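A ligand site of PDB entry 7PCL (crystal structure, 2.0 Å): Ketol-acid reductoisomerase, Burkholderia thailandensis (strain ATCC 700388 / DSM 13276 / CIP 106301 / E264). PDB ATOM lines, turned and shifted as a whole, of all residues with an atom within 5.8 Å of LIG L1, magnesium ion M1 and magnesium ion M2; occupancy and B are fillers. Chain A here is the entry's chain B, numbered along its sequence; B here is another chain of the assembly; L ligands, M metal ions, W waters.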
ATOM      1  N   GLU A 231      14.859  -7.771  30.852  1.00  0.00           N
ATOM      2  CA  GLU A 231      15.247  -7.606  29.422  1.00  0.00           C
ATOM      3  C   GLU A 231      14.242  -8.329  28.515  1.00  0.00           C
ATOM      4  O   GLU A 231      13.894  -7.753  27.475  1.00  0.00           O
ATOM      5  CB  GLU A 231      16.665  -8.116  29.179  1.00  0.00           C
ATOM      6  CG  GLU A 231      17.749  -7.231  29.757  1.00  0.00           C
ATOM      7  CD  GLU A 231      17.473  -5.741  29.658  1.00  0.00           C
ATOM      8  OE1 GLU A 231      17.455  -5.214  28.526  1.00  0.00           O
ATOM      9  OE2 GLU A 231      17.262  -5.109  30.721  1.00  0.00           O
ATOM     10  N   GLU A 237       9.912  -3.075  27.947  1.00  0.00           N
ATOM     11  CA  GLU A 237      10.551  -2.563  26.709  1.00  0.00           C
ATOM     12  C   GLU A 237      10.041  -3.345  25.493  1.00  0.00           C
ATOM     13  O   GLU A 237       9.665  -2.698  24.503  1.00  0.00           O
ATOM     14  CB  GLU A 237      12.083  -2.630  26.789  1.00  0.00           C
ATOM     15  CG  GLU A 237      12.756  -1.814  25.703  1.00  0.00           C
ATOM     16  CD  GLU A 237      14.256  -1.678  25.825  1.00  0.00           C
ATOM     17  OE1 GLU A 237      14.901  -2.617  26.344  1.00  0.00           O
ATOM     18  OE2 GLU A 237      14.784  -0.631  25.401  1.00  0.00           O
ATOM     19  N   MET A 238      10.013  -4.676  25.560  1.00  0.00           N
ATOM     20  CA  MET A 238       9.558  -5.542  24.434  1.00  0.00           C
ATOM     21  C   MET A 238       8.059  -5.308  24.186  1.00  0.00           C
ATOM     22  O   MET A 238       7.671  -5.187  23.012  1.00  0.00           O
ATOM     23  CB  MET A 238       9.837  -7.024  24.709  1.00  0.00           C
ATOM     24  CG  MET A 238      11.319  -7.375  24.714  1.00  0.00           C
ATOM     25  SD  MET A 238      12.148  -7.130  23.117  1.00  0.00           S
ATOM     26  CE  MET A 238      12.779  -5.458  23.296  1.00  0.00           C
ATOM     27  N   GLN A 257      13.805   3.918  17.070  1.00  0.00           N
ATOM     28  CA  GLN A 257      14.045   3.965  18.550  1.00  0.00           C
ATOM     29  C   GLN A 257      15.314   3.198  18.957  1.00  0.00           C
ATOM     30  O   GLN A 257      15.719   3.343  20.127  1.00  0.00           O
ATOM     31  CB  GLN A 257      12.854   3.378  19.296  1.00  0.00           C
ATOM     32  CG  GLN A 257      11.529   4.090  19.017  1.00  0.00           C
ATOM     33  CD  GLN A 257      11.464   5.463  19.644  1.00  0.00           C
ATOM     34  OE1 GLN A 257      12.475   6.067  20.002  1.00  0.00           O
ATOM     35  NE2 GLN A 257      10.248   5.970  19.799  1.00  0.00           N
ATOM     36  N   GLY A 258      15.906   2.407  18.063  1.00  0.00           N
ATOM     37  CA  GLY A 258      17.110   1.608  18.364  1.00  0.00           C
ATOM     38  C   GLY A 258      18.380   2.365  18.050  1.00  0.00           C
ATOM     39  O   GLY A 258      18.423   3.021  16.983  1.00  0.00           O
ATOM     40  N   SER A 259      19.391   2.294  18.927  1.00  0.00           N
ATOM     41  CA  SER A 259      20.772   2.750  18.637  1.00  0.00           C
ATOM     42  C   SER A 259      21.257   2.042  17.376  1.00  0.00           C
ATOM     43  O   SER A 259      20.721   1.003  16.993  1.00  0.00           O
ATOM     44  CB  SER A 259      21.702   2.485  19.803  1.00  0.00           C
ATOM     45  OG  SER A 259      22.052   1.107  19.881  1.00  0.00           O
ATOM     46  N   THR A 261      23.955   0.354  17.080  1.00  0.00           N
ATOM     47  CA  THR A 261      24.389  -0.935  17.676  1.00  0.00           C
ATOM     48  C   THR A 261      23.224  -1.918  17.664  1.00  0.00           C
ATOM     49  O   THR A 261      23.400  -3.062  17.197  1.00  0.00           O
ATOM     50  CB  THR A 261      24.903  -0.748  19.112  1.00  0.00           C
ATOM     51  OG1 THR A 261      25.874   0.302  19.094  1.00  0.00           O
ATOM     52  CG2 THR A 261      25.525  -2.004  19.690  1.00  0.00           C
ATOM     53  N   CYS A 262      22.065  -1.473  18.166  1.00  0.00           N
ATOM     54  CA  CYS A 262      20.811  -2.269  18.256  1.00  0.00           C
ATOM     55  C   CYS A 262      20.323  -2.660  16.857  1.00  0.00           C
ATOM     56  O   CYS A 262      19.992  -3.848  16.656  1.00  0.00           O
ATOM     57  CB  CYS A 262      19.723  -1.498  18.979  1.00  0.00           C
ATOM     58  SG  CYS A 262      18.094  -2.275  18.852  1.00  0.00           S
ATOM     59  N   ASP B  88      27.682   3.670  19.946  1.00  0.00           N
ATOM     60  CA  ASP B  88      28.766   2.982  20.693  1.00  0.00           C
ATOM     61  C   ASP B  88      30.058   2.927  19.879  1.00  0.00           C
ATOM     62  O   ASP B  88      31.135   3.108  20.477  1.00  0.00           O
ATOM     63  CB  ASP B  88      28.311   1.602  21.149  1.00  0.00           C
ATOM     64  CG  ASP B  88      27.095   1.703  22.046  1.00  0.00           C
ATOM     65  OD1 ASP B  88      27.277   2.049  23.229  1.00  0.00           O
ATOM     66  OD2 ASP B  88      25.976   1.473  21.549  1.00  0.00           O
ATOM     67  N   HIS B 113      25.689   2.135  28.003  1.00  0.00           N
ATOM     68  CA  HIS B 113      25.891   0.773  27.438  1.00  0.00           C
ATOM     69  C   HIS B 113      27.353   0.388  27.672  1.00  0.00           C
ATOM     70  O   HIS B 113      28.226   1.268  27.537  1.00  0.00           O
ATOM     71  CB  HIS B 113      25.456   0.766  25.964  1.00  0.00           C
ATOM     72  CG  HIS B 113      25.481  -0.572  25.295  1.00  0.00           C
ATOM     73  ND1 HIS B 113      25.076  -1.734  25.930  1.00  0.00           N
ATOM     74  CD2 HIS B 113      25.826  -0.934  24.043  1.00  0.00           C
ATOM     75  CE1 HIS B 113      25.185  -2.742  25.095  1.00  0.00           C
ATOM     76  NE2 HIS B 113      25.640  -2.285  23.933  1.00  0.00           N
ATOM     77  N   PRO B 135      19.819   2.720  30.848  1.00  0.00           N
ATOM     78  CA  PRO B 135      18.359   2.576  30.929  1.00  0.00           C
ATOM     79  C   PRO B 135      17.864   1.313  30.200  1.00  0.00           C
ATOM     80  O   PRO B 135      18.465   0.949  29.192  1.00  0.00           O
ATOM     81  CB  PRO B 135      17.823   3.838  30.233  1.00  0.00           C
ATOM     82  CG  PRO B 135      18.989   4.808  30.220  1.00  0.00           C
ATOM     83  CD  PRO B 135      20.208   3.925  30.099  1.00  0.00           C
ATOM     84  N   ARG B 136      16.796   0.695  30.705  1.00  0.00           N
ATOM     85  CA  ARG B 136      16.179  -0.534  30.128  1.00  0.00           C
ATOM     86  C   ARG B 136      14.960  -0.133  29.281  1.00  0.00           C
ATOM     87  O   ARG B 136      13.942  -0.851  29.324  1.00  0.00           O
ATOM     88  CB  ARG B 136      15.721  -1.511  31.214  1.00  0.00           C
ATOM     89  CG  ARG B 136      16.775  -1.888  32.250  1.00  0.00           C
ATOM     90  CD  ARG B 136      18.205  -1.815  31.778  1.00  0.00           C
ATOM     91  NE  ARG B 136      18.536  -2.722  30.688  1.00  0.00           N
ATOM     92  CZ  ARG B 136      19.656  -2.673  29.975  1.00  0.00           C
ATOM     93  NH1 ARG B 136      20.562  -1.737  30.215  1.00  0.00           N
ATOM     94  NH2 ARG B 136      19.870  -3.546  29.015  1.00  0.00           N
ATOM     95  N   MET B 137      15.068   0.968  28.533  1.00  0.00           N
ATOM     96  CA  MET B 137      13.933   1.616  27.827  1.00  0.00           C
ATOM     97  C   MET B 137      14.494   2.670  26.865  1.00  0.00           C
ATOM     98  O   MET B 137      15.559   3.238  27.172  1.00  0.00           O
ATOM     99  CB  MET B 137      13.008   2.302  28.841  1.00  0.00           C
ATOM    100  CG  MET B 137      11.711   2.828  28.252  1.00  0.00           C
ATOM    101  SD  MET B 137      10.691   1.561  27.454  1.00  0.00           S
ATOM    102  CE  MET B 137      10.429   0.427  28.811  1.00  0.00           C
ATOM    103  N   TYR B 138      13.774   2.941  25.766  1.00  0.00           N
ATOM    104  CA  TYR B 138      14.139   3.979  24.774  1.00  0.00           C
ATOM    105  C   TYR B 138      13.570   5.334  25.244  1.00  0.00           C
ATOM    106  O   TYR B 138      12.871   5.375  26.273  1.00  0.00           O
ATOM    107  CB  TYR B 138      13.759   3.568  23.341  1.00  0.00           C
ATOM    108  CG  TYR B 138      12.378   2.993  23.107  1.00  0.00           C
ATOM    109  CD1 TYR B 138      11.334   3.781  22.666  1.00  0.00           C
ATOM    110  CD2 TYR B 138      12.152   1.628  23.239  1.00  0.00           C
ATOM    111  CE1 TYR B 138      10.084   3.252  22.405  1.00  0.00           C
ATOM    112  CE2 TYR B 138      10.905   1.075  22.982  1.00  0.00           C
ATOM    113  CZ  TYR B 138       9.865   1.889  22.568  1.00  0.00           C
ATOM    114  OH  TYR B 138       8.639   1.358  22.309  1.00  0.00           O
ATOM    115  N   GLU B 192      25.882  -6.314  31.420  1.00  0.00           N
ATOM    116  CA  GLU B 192      24.896  -5.401  30.770  1.00  0.00           C
ATOM    117  C   GLU B 192      25.056  -5.498  29.248  1.00  0.00           C
ATOM    118  O   GLU B 192      24.043  -5.667  28.551  1.00  0.00           O
ATOM    119  CB  GLU B 192      25.057  -3.956  31.242  1.00  0.00           C
ATOM    120  CG  GLU B 192      23.941  -3.025  30.776  1.00  0.00           C
ATOM    121  CD  GLU B 192      24.043  -2.506  29.345  1.00  0.00           C
ATOM    122  OE1 GLU B 192      25.159  -2.512  28.784  1.00  0.00           O
ATOM    123  OE2 GLU B 192      22.998  -2.100  28.807  1.00  0.00           O
ATOM    124  N   ASP B 196      22.104  -6.876  26.948  1.00  0.00           N
ATOM    125  CA  ASP B 196      21.508  -5.836  26.075  1.00  0.00           C
ATOM    126  C   ASP B 196      21.581  -6.302  24.612  1.00  0.00           C
ATOM    127  O   ASP B 196      20.537  -6.275  23.944  1.00  0.00           O
ATOM    128  CB  ASP B 196      22.208  -4.495  26.276  1.00  0.00           C
ATOM    129  CG  ASP B 196      21.415  -3.316  25.731  1.00  0.00           C
ATOM    130  OD1 ASP B 196      20.378  -2.982  26.346  1.00  0.00           O
ATOM    131  OD2 ASP B 196      21.836  -2.763  24.694  1.00  0.00           O
ATOM    132  N   LEU B 197      22.766  -6.733  24.159  1.00  0.00           N
ATOM    133  CA  LEU B 197      22.986  -7.201  22.772  1.00  0.00           C
ATOM    134  C   LEU B 197      22.147  -8.462  22.512  1.00  0.00           C
ATOM    135  O   LEU B 197      21.633  -8.603  21.384  1.00  0.00           O
ATOM    136  CB  LEU B 197      24.480  -7.465  22.531  1.00  0.00           C
ATOM    137  CG  LEU B 197      25.389  -6.240  22.559  1.00  0.00           C
ATOM    138  CD1 LEU B 197      26.799  -6.603  22.126  1.00  0.00           C
ATOM    139  CD2 LEU B 197      24.851  -5.115  21.685  1.00  0.00           C
ATOM    140  N   GLN B 199      19.158  -9.224  23.807  1.00  0.00           N
ATOM    141  CA  GLN B 199      17.758  -8.762  23.624  1.00  0.00           C
ATOM    142  C   GLN B 199      17.560  -8.269  22.189  1.00  0.00           C
ATOM    143  O   GLN B 199      16.501  -8.563  21.599  1.00  0.00           O
ATOM    144  CB  GLN B 199      17.437  -7.652  24.631  1.00  0.00           C
ATOM    145  CG  GLN B 199      15.954  -7.310  24.701  1.00  0.00           C
ATOM    146  CD  GLN B 199      15.753  -5.844  25.018  1.00  0.00           C
ATOM    147  OE1 GLN B 199      16.282  -4.971  24.340  1.00  0.00           O
ATOM    148  NE2 GLN B 199      14.977  -5.571  26.057  1.00  0.00           N
ATOM    149  N   GLU B 200      18.569  -7.580  21.647  1.00  0.00           N
ATOM    150  CA  GLU B 200      18.526  -6.922  20.317  1.00  0.00           C
ATOM    151  C   GLU B 200      18.741  -7.950  19.196  1.00  0.00           C
ATOM    152  O   GLU B 200      18.173  -7.741  18.100  1.00  0.00           O
ATOM    153  CB  GLU B 200      19.588  -5.818  20.267  1.00  0.00           C
ATOM    154  CG  GLU B 200      19.324  -4.706  21.274  1.00  0.00           C
ATOM    155  CD  GLU B 200      20.502  -3.782  21.552  1.00  0.00           C
ATOM    156  OE1 GLU B 200      21.587  -4.012  20.990  1.00  0.00           O
ATOM    157  OE2 GLU B 200      20.312  -2.821  22.329  1.00  0.00           O
HETATM  158  C1  LIG L   1      16.843  -0.712  22.395  1.00  0.00           C
HETATM  159  C2  LIG L   1      16.218  -2.104  22.449  1.00  0.00           C
HETATM  160  O1  LIG L   1      18.818   0.766  21.309  1.00  0.00           O
HETATM  161  C3  LIG L   1      19.526   0.161  22.131  1.00  0.00           C
HETATM  162  O2  LIG L   1      20.701  -0.211  21.916  1.00  0.00           O
HETATM  163  C4  LIG L   1      18.983  -0.062  23.561  1.00  0.00           C
HETATM  164  O3  LIG L   1      19.747  -1.048  24.232  1.00  0.00           O
HETATM  165  N1  LIG L   1      17.514  -0.334  23.656  1.00  0.00           N
HETATM  166  O4  LIG L   1      17.186  -1.317  24.779  1.00  0.00           O
HETATM  167  C5  LIG L   1      15.739   0.303  22.077  1.00  0.00           C
HETATM  168  P1  LG2 L   2      21.418   7.718  18.300  1.00  0.00           P
HETATM  169  O1  LG2 L   2      21.660   6.952  17.060  1.00  0.00           O
HETATM  170  O2  LG2 L   2      20.071   8.281  18.519  1.00  0.00           O
HETATM  171  O3  LG2 L   2      22.515   8.868  18.458  1.00  0.00           O
HETATM  172  C1  LG2 L   2      22.444  10.064  17.659  1.00  0.00           C
HETATM  173  C2  LG2 L   2      23.318  11.124  18.294  1.00  0.00           C
HETATM  174  O4  LG2 L   2      24.707  10.724  18.233  1.00  0.00           O
HETATM  175  C3  LG2 L   2      23.245  12.521  17.656  1.00  0.00           C
HETATM  176  O5  LG2 L   2      23.346  13.515  18.662  1.00  0.00           O
HETATM  177  C4  LG2 L   2      24.472  12.517  16.736  1.00  0.00           C
HETATM  178  O6  LG2 L   2      24.980  13.801  16.478  1.00  0.00           O
HETATM  179  C5  LG2 L   2      25.458  11.704  17.565  1.00  0.00           C
HETATM  180  N1  LG2 L   2      26.509  11.075  16.771  1.00  0.00           N
HETATM  181  C6  LG2 L   2      26.334  10.126  15.805  1.00  0.00           C
HETATM  182  N2  LG2 L   2      27.455   9.746  15.246  1.00  0.00           N
HETATM  183  C7  LG2 L   2      28.433  10.495  15.894  1.00  0.00           C
HETATM  184  C8  LG2 L   2      29.825  10.543  15.749  1.00  0.00           C
HETATM  185  N3  LG2 L   2      30.510   9.807  14.878  1.00  0.00           N
HETATM  186  N4  LG2 L   2      30.501  11.399  16.549  1.00  0.00           N
HETATM  187  C9  LG2 L   2      29.809  12.146  17.414  1.00  0.00           C
HETATM  188  N5  LG2 L   2      28.498  12.172  17.636  1.00  0.00           N
HETATM  189  C10 LG2 L   2      27.852  11.322  16.826  1.00  0.00           C
HETATM  190  O7  LG2 L   2      21.863   6.841  19.546  1.00  0.00           O
HETATM  191  P2  LG2 L   2      21.156   6.319  20.873  1.00  0.00           P
HETATM  192  O8  LG2 L   2      20.216   5.237  20.499  1.00  0.00           O
HETATM  193  O9  LG2 L   2      20.633   7.496  21.621  1.00  0.00           O
HETATM  194  O10 LG2 L   2      22.377   5.704  21.676  1.00  0.00           O
HETATM  195  C11 LG2 L   2      23.213   6.535  22.509  1.00  0.00           C
HETATM  196  C12 LG2 L   2      23.862   5.673  23.572  1.00  0.00           C
HETATM  197  O11 LG2 L   2      22.825   5.209  24.467  1.00  0.00           O
HETATM  198  C13 LG2 L   2      24.576   4.415  23.051  1.00  0.00           C
HETATM  199  O12 LG2 L   2      25.748   4.165  23.801  1.00  0.00           O
HETATM  200  C14 LG2 L   2      23.489   3.345  23.218  1.00  0.00           C
HETATM  201  O13 LG2 L   2      24.026   2.039  23.321  1.00  0.00           O
HETATM  202  C15 LG2 L   2      22.830   3.793  24.521  1.00  0.00           C
HETATM  203  N6  LG2 L   2      21.438   3.303  24.686  1.00  0.00           N
HETATM  204  C16 LG2 L   2      20.501   3.488  23.700  1.00  0.00           C
HETATM  205  C17 LG2 L   2      19.175   3.141  23.931  1.00  0.00           C
HETATM  206  C18 LG2 L   2      18.115   3.502  22.927  1.00  0.00           C
HETATM  207  O14 LG2 L   2      16.939   3.401  23.230  1.00  0.00           O
HETATM  208  N7  LG2 L   2      18.510   3.953  21.742  1.00  0.00           N
HETATM  209  C19 LG2 L   2      18.847   2.505  25.121  1.00  0.00           C
HETATM  210  C20 LG2 L   2      19.777   2.426  26.125  1.00  0.00           C
HETATM  211  C21 LG2 L   2      21.093   2.679  25.830  1.00  0.00           C
HETATM  212 MG    MG M   1      18.687  -1.975  25.785  1.00  0.00          MG
HETATM  213 MG    MG M   2      21.632  -1.393  23.341  1.00  0.00          MG
HETATM  214  O   HOH W   1      22.510   0.112  24.428  1.00  0.00           O
HETATM  215  O   HOH W   2      18.480  -3.522  24.338  1.00  0.00           O
HETATM  216  O   HOH W   3      23.132  -2.011  21.910  1.00  0.00           O
HETATM  217  O   HOH W   4      17.386  -2.975  27.037  1.00  0.00           O
HETATM  218  O   HOH W   5      19.415  -0.644  27.268  1.00  0.00           O
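An oxygen (O1) of LIG L1 is in hydrogen-bond range of a nitrogen (N7) of LG2 L2, at 3.2 Å.
The backbone NH (N) of Thr 261 sits close to the side-chain hydroxyl (OG) of Ser 259. The side-chain hydroxyl of Ser 259 lies within hydrogen-bond range of the backbone NH of Cys 262. NH1 of Arg 136 of chain B is in salt-bridge range of OE2 of Glu 192 of chain B. The side-chain carboxylate (OE1) of Glu 237 sits at hydrogen-bond distance from the side-chain amide nitrogen (NE2) of Gln 199 of chain B. NE2 of Gln 199 of chain B lies within hydrogen-bond range of O of Glu 231, 2.8 Å away. The side-chain carboxylate (OE2) of Glu 231 lies within salt-bridge range of the guanidinium group (NE) of Arg 136 of chain B (2.7 Å). NH2 of Arg 136 of chain B sits close to OD1 of Asp 196 of chain B, 2.8 Å away.
Magnesium ion M1 is bound by an oxygen (O4) of LIG L1 (1.9 Å), the side-chain carboxylate of Asp 196 of chain B (2.0 Å), water W4 (2.1 Å), an oxygen (O3) of LIG L1 (2.1 Å), water W5 (2.1 Å) and water W2 (2.1 Å). Magnesium ion M1 has six donor atoms within binding distance.
Within 4 Å of magnesium ion M2: Asp 196 of chain B and Glu 200 of chain B.
Water W4 lies within hydrogen-bond range of OE1 of Glu 237 (2.6 Å), OE1 of Glu 231 (2.7 Å) and NH2 of Arg 136 of chain B (3.2 Å). Water W5 lies within hydrogen-bond range of O of Pro 135 of chain B and NH1 of Arg 136 of chain B. Water W2 lies within hydrogen-bond range of the side-chain amide oxygen of Gln 199 of chain B and the backbone carbonyl oxygen of Asp 196 of chain B. Water W3 bridges OE1 of Glu 200 of chain B (2.7 Å) and NE2 of His 113 of chain B (3.2 Å).
The side-chain carboxylate of Asp 88 of chain B sits at hydrogen-bond distance from an oxygen (O12) of LG2 L2, 2.7 Å away. The backbone NH (N) of Ser 259 sits at hydrogen-bond distance from an oxygen (O1) of LIG L1, 2.9 Å away. A nitrogen (N7) of LG2 L2 lies within hydrogen-bond range of the backbone carbonyl oxygen (O) of Gln 257, at 3.3 Å. The side-chain hydroxyl (OG) of Ser 259 lies close to an oxygen (O2) of LIG L1. An oxygen (O4) of LIG L1 sits close to the side-chain carboxylate (OE2) of Glu 237, at 2.6 Å. The backbone NH (N) of Ser 259 lies close to an oxygen (O8) of LG2 L2, 3.4 Å away.
Residues that only touch magnesium ion M1: Glu 237 and Arg 136 of chain B. Four residues have an atom within 4 Å of magnesium ion M1: Glu 237, Arg 136 of chain B, Asp 196 of chain B and Glu 200 of chain B.
Magnesium ion M2 is bound by OD2 of Asp 196 of chain B, water W1, O2 of LIG L1, O3 of LIG L1, water W3 and OE2 of Glu 200 of chain B.
O of Gln 257 touches C5 of LIG L1, at 3.6 Å. Gly 258 touches LIG L1 (CA to O1, 3.5 Å). Cys 262 touches LIG L1 (CB to O2, 3.4 Å). Tyr 138 of chain B touches LIG L1. Gln 199 of chain B touches LIG L1. Within 4 Å of LIG L1: Glu 237, Gln 257, Gly 258, Ser 259, Cys 262, Tyr 138 of chain B, Asp 196 of chain B, Gln 199 of chain B and Glu 200 of chain B.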
